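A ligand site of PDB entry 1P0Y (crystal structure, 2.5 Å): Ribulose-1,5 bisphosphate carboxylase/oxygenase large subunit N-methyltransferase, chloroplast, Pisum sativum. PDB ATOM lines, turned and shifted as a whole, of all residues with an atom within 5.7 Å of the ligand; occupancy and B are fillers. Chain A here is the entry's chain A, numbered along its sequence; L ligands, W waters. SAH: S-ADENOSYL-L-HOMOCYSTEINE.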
ATOM      1  N   VAL A  34      22.981  -7.129 -28.624  1.00  0.00           N
ATOM      2  CA  VAL A  34      22.411  -6.214 -29.596  1.00  0.00           C
ATOM      3  C   VAL A  34      23.499  -5.454 -30.333  1.00  0.00           C
ATOM      4  O   VAL A  34      24.663  -5.489 -29.946  1.00  0.00           O
ATOM      5  CB  VAL A  34      21.452  -5.205 -28.935  1.00  0.00           C
ATOM      6  CG1 VAL A  34      20.241  -5.941 -28.384  1.00  0.00           C
ATOM      7  CG2 VAL A  34      22.169  -4.452 -27.836  1.00  0.00           C
ATOM      8  N   GLU A  36      24.270  -2.494 -30.304  1.00  0.00           N
ATOM      9  CA  GLU A  36      24.979  -1.590 -29.421  1.00  0.00           C
ATOM     10  C   GLU A  36      25.713  -2.272 -28.269  1.00  0.00           C
ATOM     11  O   GLU A  36      25.932  -1.663 -27.214  1.00  0.00           O
ATOM     12  CB  GLU A  36      24.021  -0.533 -28.862  1.00  0.00           C
ATOM     13  CG  GLU A  36      22.657  -1.088 -28.474  1.00  0.00           C
ATOM     14  CD  GLU A  36      21.690  -1.150 -29.641  1.00  0.00           C
ATOM     15  OE1 GLU A  36      21.051  -0.109 -29.943  1.00  0.00           O
ATOM     16  OE2 GLU A  36      21.564  -2.233 -30.255  1.00  0.00           O
ATOM     17  N   GLY A  37      26.111  -3.529 -28.472  1.00  0.00           N
ATOM     18  CA  GLY A  37      26.823  -4.265 -27.449  1.00  0.00           C
ATOM     19  C   GLY A  37      25.946  -5.260 -26.705  1.00  0.00           C
ATOM     20  O   GLY A  37      25.653  -6.356 -27.211  1.00  0.00           O
ATOM     21  N   LEU A  38      25.538  -4.888 -25.500  1.00  0.00           N
ATOM     22  CA  LEU A  38      24.663  -5.727 -24.680  1.00  0.00           C
ATOM     23  C   LEU A  38      23.466  -4.883 -24.305  1.00  0.00           C
ATOM     24  O   LEU A  38      23.602  -3.694 -23.985  1.00  0.00           O
ATOM     25  CB  LEU A  38      25.377  -6.180 -23.398  1.00  0.00           C
ATOM     26  CG  LEU A  38      26.317  -7.377 -23.509  1.00  0.00           C
ATOM     27  CD1 LEU A  38      27.084  -7.547 -22.209  1.00  0.00           C
ATOM     28  CD2 LEU A  38      25.495  -8.619 -23.828  1.00  0.00           C
ATOM     29  N   GLY A  39      22.283  -5.471 -24.342  1.00  0.00           N
ATOM     30  CA  GLY A  39      21.104  -4.705 -24.009  1.00  0.00           C
ATOM     31  C   GLY A  39      20.042  -5.556 -23.366  1.00  0.00           C
ATOM     32  O   GLY A  39      20.229  -6.753 -23.145  1.00  0.00           O
ATOM     33  N   ILE A 105      31.462  -8.184 -16.587  1.00  0.00           N
ATOM     34  CA  ILE A 105      30.667  -7.888 -17.771  1.00  0.00           C
ATOM     35  C   ILE A 105      31.070  -6.560 -18.439  1.00  0.00           C
ATOM     36  O   ILE A 105      30.957  -6.415 -19.656  1.00  0.00           O
ATOM     37  CB  ILE A 105      29.153  -7.845 -17.411  1.00  0.00           C
ATOM     38  CG1 ILE A 105      28.647  -9.274 -17.235  1.00  0.00           C
ATOM     39  CG2 ILE A 105      28.353  -7.163 -18.475  1.00  0.00           C
ATOM     40  CD1 ILE A 105      28.873 -10.140 -18.468  1.00  0.00           C
ATOM     41  N   PRO A 107      32.615  -3.784 -20.421  1.00  0.00           N
ATOM     42  CA  PRO A 107      33.501  -3.776 -21.588  1.00  0.00           C
ATOM     43  C   PRO A 107      34.738  -3.010 -21.152  1.00  0.00           C
ATOM     44  O   PRO A 107      34.631  -1.999 -20.448  1.00  0.00           O
ATOM     45  CB  PRO A 107      32.695  -3.008 -22.626  1.00  0.00           C
ATOM     46  CG  PRO A 107      31.272  -3.277 -22.223  1.00  0.00           C
ATOM     47  CD  PRO A 107      31.337  -3.115 -20.740  1.00  0.00           C
ATOM     48  N   THR A 110      34.912   1.721 -24.456  1.00  0.00           N
ATOM     49  CA  THR A 110      33.736   2.156 -25.217  1.00  0.00           C
ATOM     50  C   THR A 110      34.344   2.914 -26.389  1.00  0.00           C
ATOM     51  O   THR A 110      35.555   2.884 -26.569  1.00  0.00           O
ATOM     52  CB  THR A 110      32.824   3.138 -24.426  1.00  0.00           C
ATOM     53  OG1 THR A 110      33.528   4.368 -24.192  1.00  0.00           O
ATOM     54  CG2 THR A 110      32.390   2.534 -23.089  1.00  0.00           C
ATOM     55  N   ASP A 111      33.514   3.584 -27.192  1.00  0.00           N
ATOM     56  CA  ASP A 111      34.078   4.311 -28.329  1.00  0.00           C
ATOM     57  C   ASP A 111      34.289   5.776 -28.025  1.00  0.00           C
ATOM     58  O   ASP A 111      34.467   6.592 -28.933  1.00  0.00           O
ATOM     59  CB  ASP A 111      33.206   4.131 -29.573  1.00  0.00           C
ATOM     60  CG  ASP A 111      33.430   2.784 -30.243  1.00  0.00           C
ATOM     61  OD1 ASP A 111      34.603   2.365 -30.342  1.00  0.00           O
ATOM     62  OD2 ASP A 111      32.444   2.154 -30.669  1.00  0.00           O
ATOM     63  N   SER A 177      29.857   6.863 -18.677  1.00  0.00           N
ATOM     64  CA  SER A 177      28.996   6.283 -19.695  1.00  0.00           C
ATOM     65  C   SER A 177      27.884   5.428 -19.098  1.00  0.00           C
ATOM     66  O   SER A 177      26.987   4.980 -19.812  1.00  0.00           O
ATOM     67  CB  SER A 177      29.818   5.436 -20.668  1.00  0.00           C
ATOM     68  OG  SER A 177      30.389   4.301 -20.042  1.00  0.00           O
ATOM     69  N   ARG A 178      27.923   5.206 -17.788  1.00  0.00           N
ATOM     70  CA  ARG A 178      26.932   4.361 -17.131  1.00  0.00           C
ATOM     71  C   ARG A 178      26.210   4.942 -15.937  1.00  0.00           C
ATOM     72  O   ARG A 178      25.117   4.495 -15.601  1.00  0.00           O
ATOM     73  CB  ARG A 178      27.607   3.060 -16.714  1.00  0.00           C
ATOM     74  CG  ARG A 178      28.269   2.351 -17.847  1.00  0.00           C
ATOM     75  CD  ARG A 178      28.893   1.056 -17.381  1.00  0.00           C
ATOM     76  NE  ARG A 178      29.117   0.175 -18.515  1.00  0.00           N
ATOM     77  CZ  ARG A 178      28.301  -0.806 -18.901  1.00  0.00           C
ATOM     78  NH1 ARG A 178      27.175  -1.063 -18.236  1.00  0.00           N
ATOM     79  NH2 ARG A 178      28.596  -1.523 -19.978  1.00  0.00           N
ATOM     80  N   ASP A 195      22.101  -0.885 -16.012  1.00  0.00           N
ATOM     81  CA  ASP A 195      23.325  -0.448 -16.651  1.00  0.00           C
ATOM     82  C   ASP A 195      23.417  -0.995 -18.063  1.00  0.00           C
ATOM     83  O   ASP A 195      24.331  -0.668 -18.814  1.00  0.00           O
ATOM     84  CB  ASP A 195      24.513  -0.964 -15.838  1.00  0.00           C
ATOM     85  CG  ASP A 195      25.675  -0.034 -15.868  1.00  0.00           C
ATOM     86  OD1 ASP A 195      25.454   1.189 -15.724  1.00  0.00           O
ATOM     87  OD2 ASP A 195      26.805  -0.527 -16.023  1.00  0.00           O
ATOM     88  N   LEU A 196      22.451  -1.835 -18.432  1.00  0.00           N
ATOM     89  CA  LEU A 196      22.436  -2.456 -19.746  1.00  0.00           C
ATOM     90  C   LEU A 196      21.416  -1.878 -20.713  1.00  0.00           C
ATOM     91  O   LEU A 196      21.407  -2.236 -21.889  1.00  0.00           O
ATOM     92  CB  LEU A 196      22.221  -3.963 -19.603  1.00  0.00           C
ATOM     93  CG  LEU A 196      23.295  -4.674 -18.778  1.00  0.00           C
ATOM     94  CD1 LEU A 196      22.881  -6.118 -18.547  1.00  0.00           C
ATOM     95  CD2 LEU A 196      24.636  -4.592 -19.513  1.00  0.00           C
ATOM     96  N   ILE A 197      20.541  -1.006 -20.231  1.00  0.00           N
ATOM     97  CA  ILE A 197      19.553  -0.423 -21.109  1.00  0.00           C
ATOM     98  C   ILE A 197      20.247   0.626 -21.968  1.00  0.00           C
ATOM     99  O   ILE A 197      20.848   1.574 -21.444  1.00  0.00           O
ATOM    100  CB  ILE A 197      18.408   0.220 -20.324  1.00  0.00           C
ATOM    101  CG1 ILE A 197      17.644  -0.877 -19.570  1.00  0.00           C
ATOM    102  CG2 ILE A 197      17.471   0.963 -21.261  1.00  0.00           C
ATOM    103  CD1 ILE A 197      16.419  -0.394 -18.860  1.00  0.00           C
ATOM    104  N   ASN A 198      20.181   0.425 -23.279  1.00  0.00           N
ATOM    105  CA  ASN A 198      20.823   1.322 -24.224  1.00  0.00           C
ATOM    106  C   ASN A 198      19.976   2.547 -24.570  1.00  0.00           C
ATOM    107  O   ASN A 198      18.807   2.645 -24.197  1.00  0.00           O
ATOM    108  CB  ASN A 198      21.186   0.553 -25.484  1.00  0.00           C
ATOM    109  CG  ASN A 198      22.245  -0.488 -25.221  1.00  0.00           C
ATOM    110  OD1 ASN A 198      23.341  -0.165 -24.783  1.00  0.00           O
ATOM    111  ND2 ASN A 198      21.920  -1.751 -25.483  1.00  0.00           N
ATOM    112  N   HIS A 199      20.600   3.474 -25.304  1.00  0.00           N
ATOM    113  CA  HIS A 199      19.954   4.725 -25.715  1.00  0.00           C
ATOM    114  C   HIS A 199      19.252   4.622 -27.064  1.00  0.00           C
ATOM    115  O   HIS A 199      19.647   3.848 -27.931  1.00  0.00           O
ATOM    116  CB  HIS A 199      21.007   5.838 -25.769  1.00  0.00           C
ATOM    117  CG  HIS A 199      20.517   7.107 -26.397  1.00  0.00           C
ATOM    118  ND1 HIS A 199      19.823   8.070 -25.691  1.00  0.00           N
ATOM    119  CD2 HIS A 199      20.634   7.574 -27.656  1.00  0.00           C
ATOM    120  CE1 HIS A 199      19.536   9.071 -26.499  1.00  0.00           C
ATOM    121  NE2 HIS A 199      20.016   8.796 -27.701  1.00  0.00           N
ATOM    122  N   SER A 200      18.214   5.428 -27.231  1.00  0.00           N
ATOM    123  CA  SER A 200      17.452   5.455 -28.459  1.00  0.00           C
ATOM    124  C   SER A 200      16.797   6.805 -28.702  1.00  0.00           C
ATOM    125  O   SER A 200      16.148   7.362 -27.798  1.00  0.00           O
ATOM    126  CB  SER A 200      16.387   4.382 -28.434  1.00  0.00           C
ATOM    127  OG  SER A 200      15.569   4.528 -29.569  1.00  0.00           O
ATOM    128  N   TYR A 240      14.654   0.611 -24.530  1.00  0.00           N
ATOM    129  CA  TYR A 240      15.567   1.735 -24.560  1.00  0.00           C
ATOM    130  C   TYR A 240      15.118   2.858 -23.641  1.00  0.00           C
ATOM    131  O   TYR A 240      14.065   2.788 -23.016  1.00  0.00           O
ATOM    132  CB  TYR A 240      15.686   2.315 -25.983  1.00  0.00           C
ATOM    133  CG  TYR A 240      16.350   1.449 -27.036  1.00  0.00           C
ATOM    134  CD1 TYR A 240      15.600   0.726 -27.964  1.00  0.00           C
ATOM    135  CD2 TYR A 240      17.738   1.403 -27.145  1.00  0.00           C
ATOM    136  CE1 TYR A 240      16.220  -0.013 -28.972  1.00  0.00           C
ATOM    137  CE2 TYR A 240      18.362   0.661 -28.144  1.00  0.00           C
ATOM    138  CZ  TYR A 240      17.599  -0.037 -29.059  1.00  0.00           C
ATOM    139  OH  TYR A 240      18.249  -0.728 -30.067  1.00  0.00           O
ATOM    140  N   TYR A 243      19.123   8.921 -23.042  1.00  0.00           N
ATOM    141  CA  TYR A 243      20.240   9.253 -22.167  1.00  0.00           C
ATOM    142  C   TYR A 243      20.242  10.731 -21.818  1.00  0.00           C
ATOM    143  O   TYR A 243      20.361  11.088 -20.649  1.00  0.00           O
ATOM    144  CB  TYR A 243      21.577   8.859 -22.803  1.00  0.00           C
ATOM    145  CG  TYR A 243      21.912   7.380 -22.684  1.00  0.00           C
ATOM    146  CD1 TYR A 243      23.147   6.894 -23.081  1.00  0.00           C
ATOM    147  CD2 TYR A 243      20.966   6.473 -22.192  1.00  0.00           C
ATOM    148  CE1 TYR A 243      23.452   5.532 -23.007  1.00  0.00           C
ATOM    149  CE2 TYR A 243      21.256   5.103 -22.101  1.00  0.00           C
ATOM    150  CZ  TYR A 243      22.498   4.646 -22.516  1.00  0.00           C
ATOM    151  OH  TYR A 243      22.787   3.294 -22.443  1.00  0.00           O
ATOM    152  N   ASP A 255      30.880  11.311 -23.735  1.00  0.00           N
ATOM    153  CA  ASP A 255      30.242  10.612 -22.624  1.00  0.00           C
ATOM    154  C   ASP A 255      29.947   9.140 -22.889  1.00  0.00           C
ATOM    155  O   ASP A 255      30.090   8.311 -22.000  1.00  0.00           O
ATOM    156  CB  ASP A 255      28.977  11.366 -22.207  1.00  0.00           C
ATOM    157  CG  ASP A 255      29.286  12.774 -21.726  1.00  0.00           C
ATOM    158  OD1 ASP A 255      28.367  13.610 -21.587  1.00  0.00           O
ATOM    159  OD2 ASP A 255      30.488  13.029 -21.471  1.00  0.00           O
ATOM    160  N   TYR A 256      29.544   8.808 -24.112  1.00  0.00           N
ATOM    161  CA  TYR A 256      29.278   7.407 -24.474  1.00  0.00           C
ATOM    162  C   TYR A 256      29.950   7.237 -25.817  1.00  0.00           C
ATOM    163  O   TYR A 256      30.431   8.211 -26.392  1.00  0.00           O
ATOM    164  CB  TYR A 256      27.785   7.141 -24.596  1.00  0.00           C
ATOM    165  CG  TYR A 256      26.950   7.896 -23.584  1.00  0.00           C
ATOM    166  CD1 TYR A 256      26.480   9.174 -23.866  1.00  0.00           C
ATOM    167  CD2 TYR A 256      26.640   7.339 -22.349  1.00  0.00           C
ATOM    168  CE1 TYR A 256      25.717   9.884 -22.935  1.00  0.00           C
ATOM    169  CE2 TYR A 256      25.882   8.037 -21.413  1.00  0.00           C
ATOM    170  CZ  TYR A 256      25.428   9.314 -21.714  1.00  0.00           C
ATOM    171  OH  TYR A 256      24.639   9.998 -20.812  1.00  0.00           O
ATOM    172  N   GLY A 257      29.998   6.024 -26.344  1.00  0.00           N
ATOM    173  CA  GLY A 257      30.667   5.897 -27.629  1.00  0.00           C
ATOM    174  C   GLY A 257      29.802   6.078 -28.857  1.00  0.00           C
ATOM    175  O   GLY A 257      29.970   5.333 -29.825  1.00  0.00           O
ATOM    176  N   PHE A 258      28.883   7.054 -28.839  1.00  0.00           N
ATOM    177  CA  PHE A 258      27.986   7.256 -29.990  1.00  0.00           C
ATOM    178  C   PHE A 258      27.485   8.677 -30.207  1.00  0.00           C
ATOM    179  O   PHE A 258      27.603   9.536 -29.331  1.00  0.00           O
ATOM    180  CB  PHE A 258      26.772   6.333 -29.854  1.00  0.00           C
ATOM    181  CG  PHE A 258      25.763   6.805 -28.827  1.00  0.00           C
ATOM    182  CD1 PHE A 258      24.933   7.897 -29.092  1.00  0.00           C
ATOM    183  CD2 PHE A 258      25.642   6.166 -27.601  1.00  0.00           C
ATOM    184  CE1 PHE A 258      24.013   8.330 -28.152  1.00  0.00           C
ATOM    185  CE2 PHE A 258      24.713   6.596 -26.658  1.00  0.00           C
ATOM    186  CZ  PHE A 258      23.904   7.675 -26.937  1.00  0.00           C
HETATM  187  N   SAH L   1      25.640  -1.688 -24.383  1.00  0.00           N
HETATM  188  CA  SAH L   1      26.361  -1.606 -23.117  1.00  0.00           C
HETATM  189  CB  SAH L   1      25.359  -1.262 -21.969  1.00  0.00           C
HETATM  190  CG  SAH L   1      24.834   0.144 -21.973  1.00  0.00           C
HETATM  191  SD  SAH L   1      25.864   1.398 -21.134  1.00  0.00           S
HETATM  192  C   SAH L   1      27.141  -2.941 -22.826  1.00  0.00           C
HETATM  193  O   SAH L   1      27.599  -3.173 -21.682  1.00  0.00           O
HETATM  194  OXT SAH L   1      27.330  -3.765 -23.746  1.00  0.00           O
HETATM  195  C5' SAH L   1      26.039   2.534 -22.488  1.00  0.00           C
HETATM  196  C4' SAH L   1      27.133   2.184 -23.487  1.00  0.00           C
HETATM  197  O4' SAH L   1      26.627   1.254 -24.472  1.00  0.00           O
HETATM  198  C3' SAH L   1      27.644   3.370 -24.279  1.00  0.00           C
HETATM  199  O3' SAH L   1      28.803   3.929 -23.691  1.00  0.00           O
HETATM  200  C2' SAH L   1      27.920   2.811 -25.656  1.00  0.00           C
HETATM  201  O2' SAH L   1      29.217   2.323 -25.866  1.00  0.00           O
HETATM  202  C1' SAH L   1      26.822   1.773 -25.777  1.00  0.00           C
HETATM  203  N9  SAH L   1      25.531   2.322 -26.339  1.00  0.00           N
HETATM  204  C8  SAH L   1      24.332   2.598 -25.698  1.00  0.00           C
HETATM  205  N7  SAH L   1      23.395   3.061 -26.484  1.00  0.00           N
HETATM  206  C5  SAH L   1      23.992   3.103 -27.734  1.00  0.00           C
HETATM  207  C6  SAH L   1      23.529   3.510 -29.011  1.00  0.00           C
HETATM  208  N6  SAH L   1      22.300   3.968 -29.228  1.00  0.00           N
HETATM  209  N1  SAH L   1      24.391   3.434 -30.075  1.00  0.00           N
HETATM  210  C2  SAH L   1      25.650   2.966 -29.875  1.00  0.00           C
HETATM  211  N3  SAH L   1      26.214   2.554 -28.716  1.00  0.00           N
HETATM  212  C4  SAH L   1      25.319   2.650 -27.664  1.00  0.00           C
HETATM  213  O   HOH W   1      28.445  -4.488 -19.332  1.00  0.00           O
HETATM  214  O   HOH W   2      24.017   5.255 -32.532  1.00  0.00           O
HETATM  215  O   HOH W   3      30.222   0.268 -23.897  1.00  0.00           O
HETATM  216  O   HOH W   4      30.722   3.137 -27.673  1.00  0.00           O
HETATM  217  O   HOH W   5      28.343   0.399 -28.797  1.00  0.00           O
HETATM  218  O   HOH W   6      19.547   2.376 -30.521  1.00  0.00           O
HETATM  219  O   HOH W   7      29.616  -4.544 -24.776  1.00  0.00           O
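The guanidinium group (NH2) of Arg 178 is in salt-bridge range of an oxygen (O) of the ligand (2.6 Å). An oxygen (OXT) of the ligand is in hydrogen-bond range of the backbone NH (N) of Leu 38. N of the ligand is in hydrogen-bond range of O of Leu 38, at 2.9 Å. The side-chain amide oxygen (OD1) of Asn 198 sits at hydrogen-bond distance from a nitrogen (N) of the ligand (2.8 Å). A nitrogen (N) of the ligand sits at hydrogen-bond distance from the backbone carbonyl oxygen of Glu 36. The backbone NH of His 199 sits at hydrogen-bond distance from a nitrogen (N7) of the ligand (3.1 Å). The backbone carbonyl oxygen of His 199 is in hydrogen-bond range of a nitrogen (N6) of the ligand (3.0 Å).
The backbone carbonyl oxygen of Asp 195 lies close to a sulfur (SD) of the ligand, at 3.5 Å. Gly 37 touches the ligand. Pro 107 touches the ligand. Thr 110 touches the ligand. Ser 177 touches the ligand. Leu 196 touches the ligand (CA to CB, 3.9 Å). Tyr 243 touches the ligand (OH to C5', 3.3 Å). Tyr 256 touches the ligand. Gly 257 touches the ligand. CD2 of Phe 258 touches C5 of the ligand (3.5 Å). Hydrophobic or aromatic side chains within 4 Å of the ligand: Leu 38, Pro 107, Leu 196, His 199, Tyr 243, Tyr 256 and Phe 258. Of the 23 residues printed, 15 come within 4 Å of the ligand. The nearest printed residue that does not touch the ligand is Ile 197 (4.3 Å).
NE of Arg 178 is in salt-bridge range of OD2 of Asp 195. O of Leu 38 lies within hydrogen-bond range of ND2 of Asn 198 (3.0 Å). OE1 of Glu 36 sits at hydrogen-bond distance from OH of Tyr 240 (2.9 Å). A ring nitrogen (ND1) of His 199 lies within hydrogen-bond range of the backbone NH of Tyr 243 (2.9 Å). OH of Tyr 243 sits at hydrogen-bond distance from O of Ile 197, at 2.8 Å.
Water W4 lies within hydrogen-bond range of an oxygen (O2') of the ligand, the backbone NH of Asp 111 and the backbone carbonyl oxygen of Gly 257. Water W1 lies within hydrogen-bond range of O of the ligand, NH2 of Arg 178 and O of Ile 105. Water W6 lies within hydrogen-bond range of the side-chain carboxylate (OE1) of Glu 36, the backbone carbonyl oxygen (O) of His 199, the side-chain hydroxyl (OH) of Tyr 240 and a nitrogen (N6) of the ligand.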
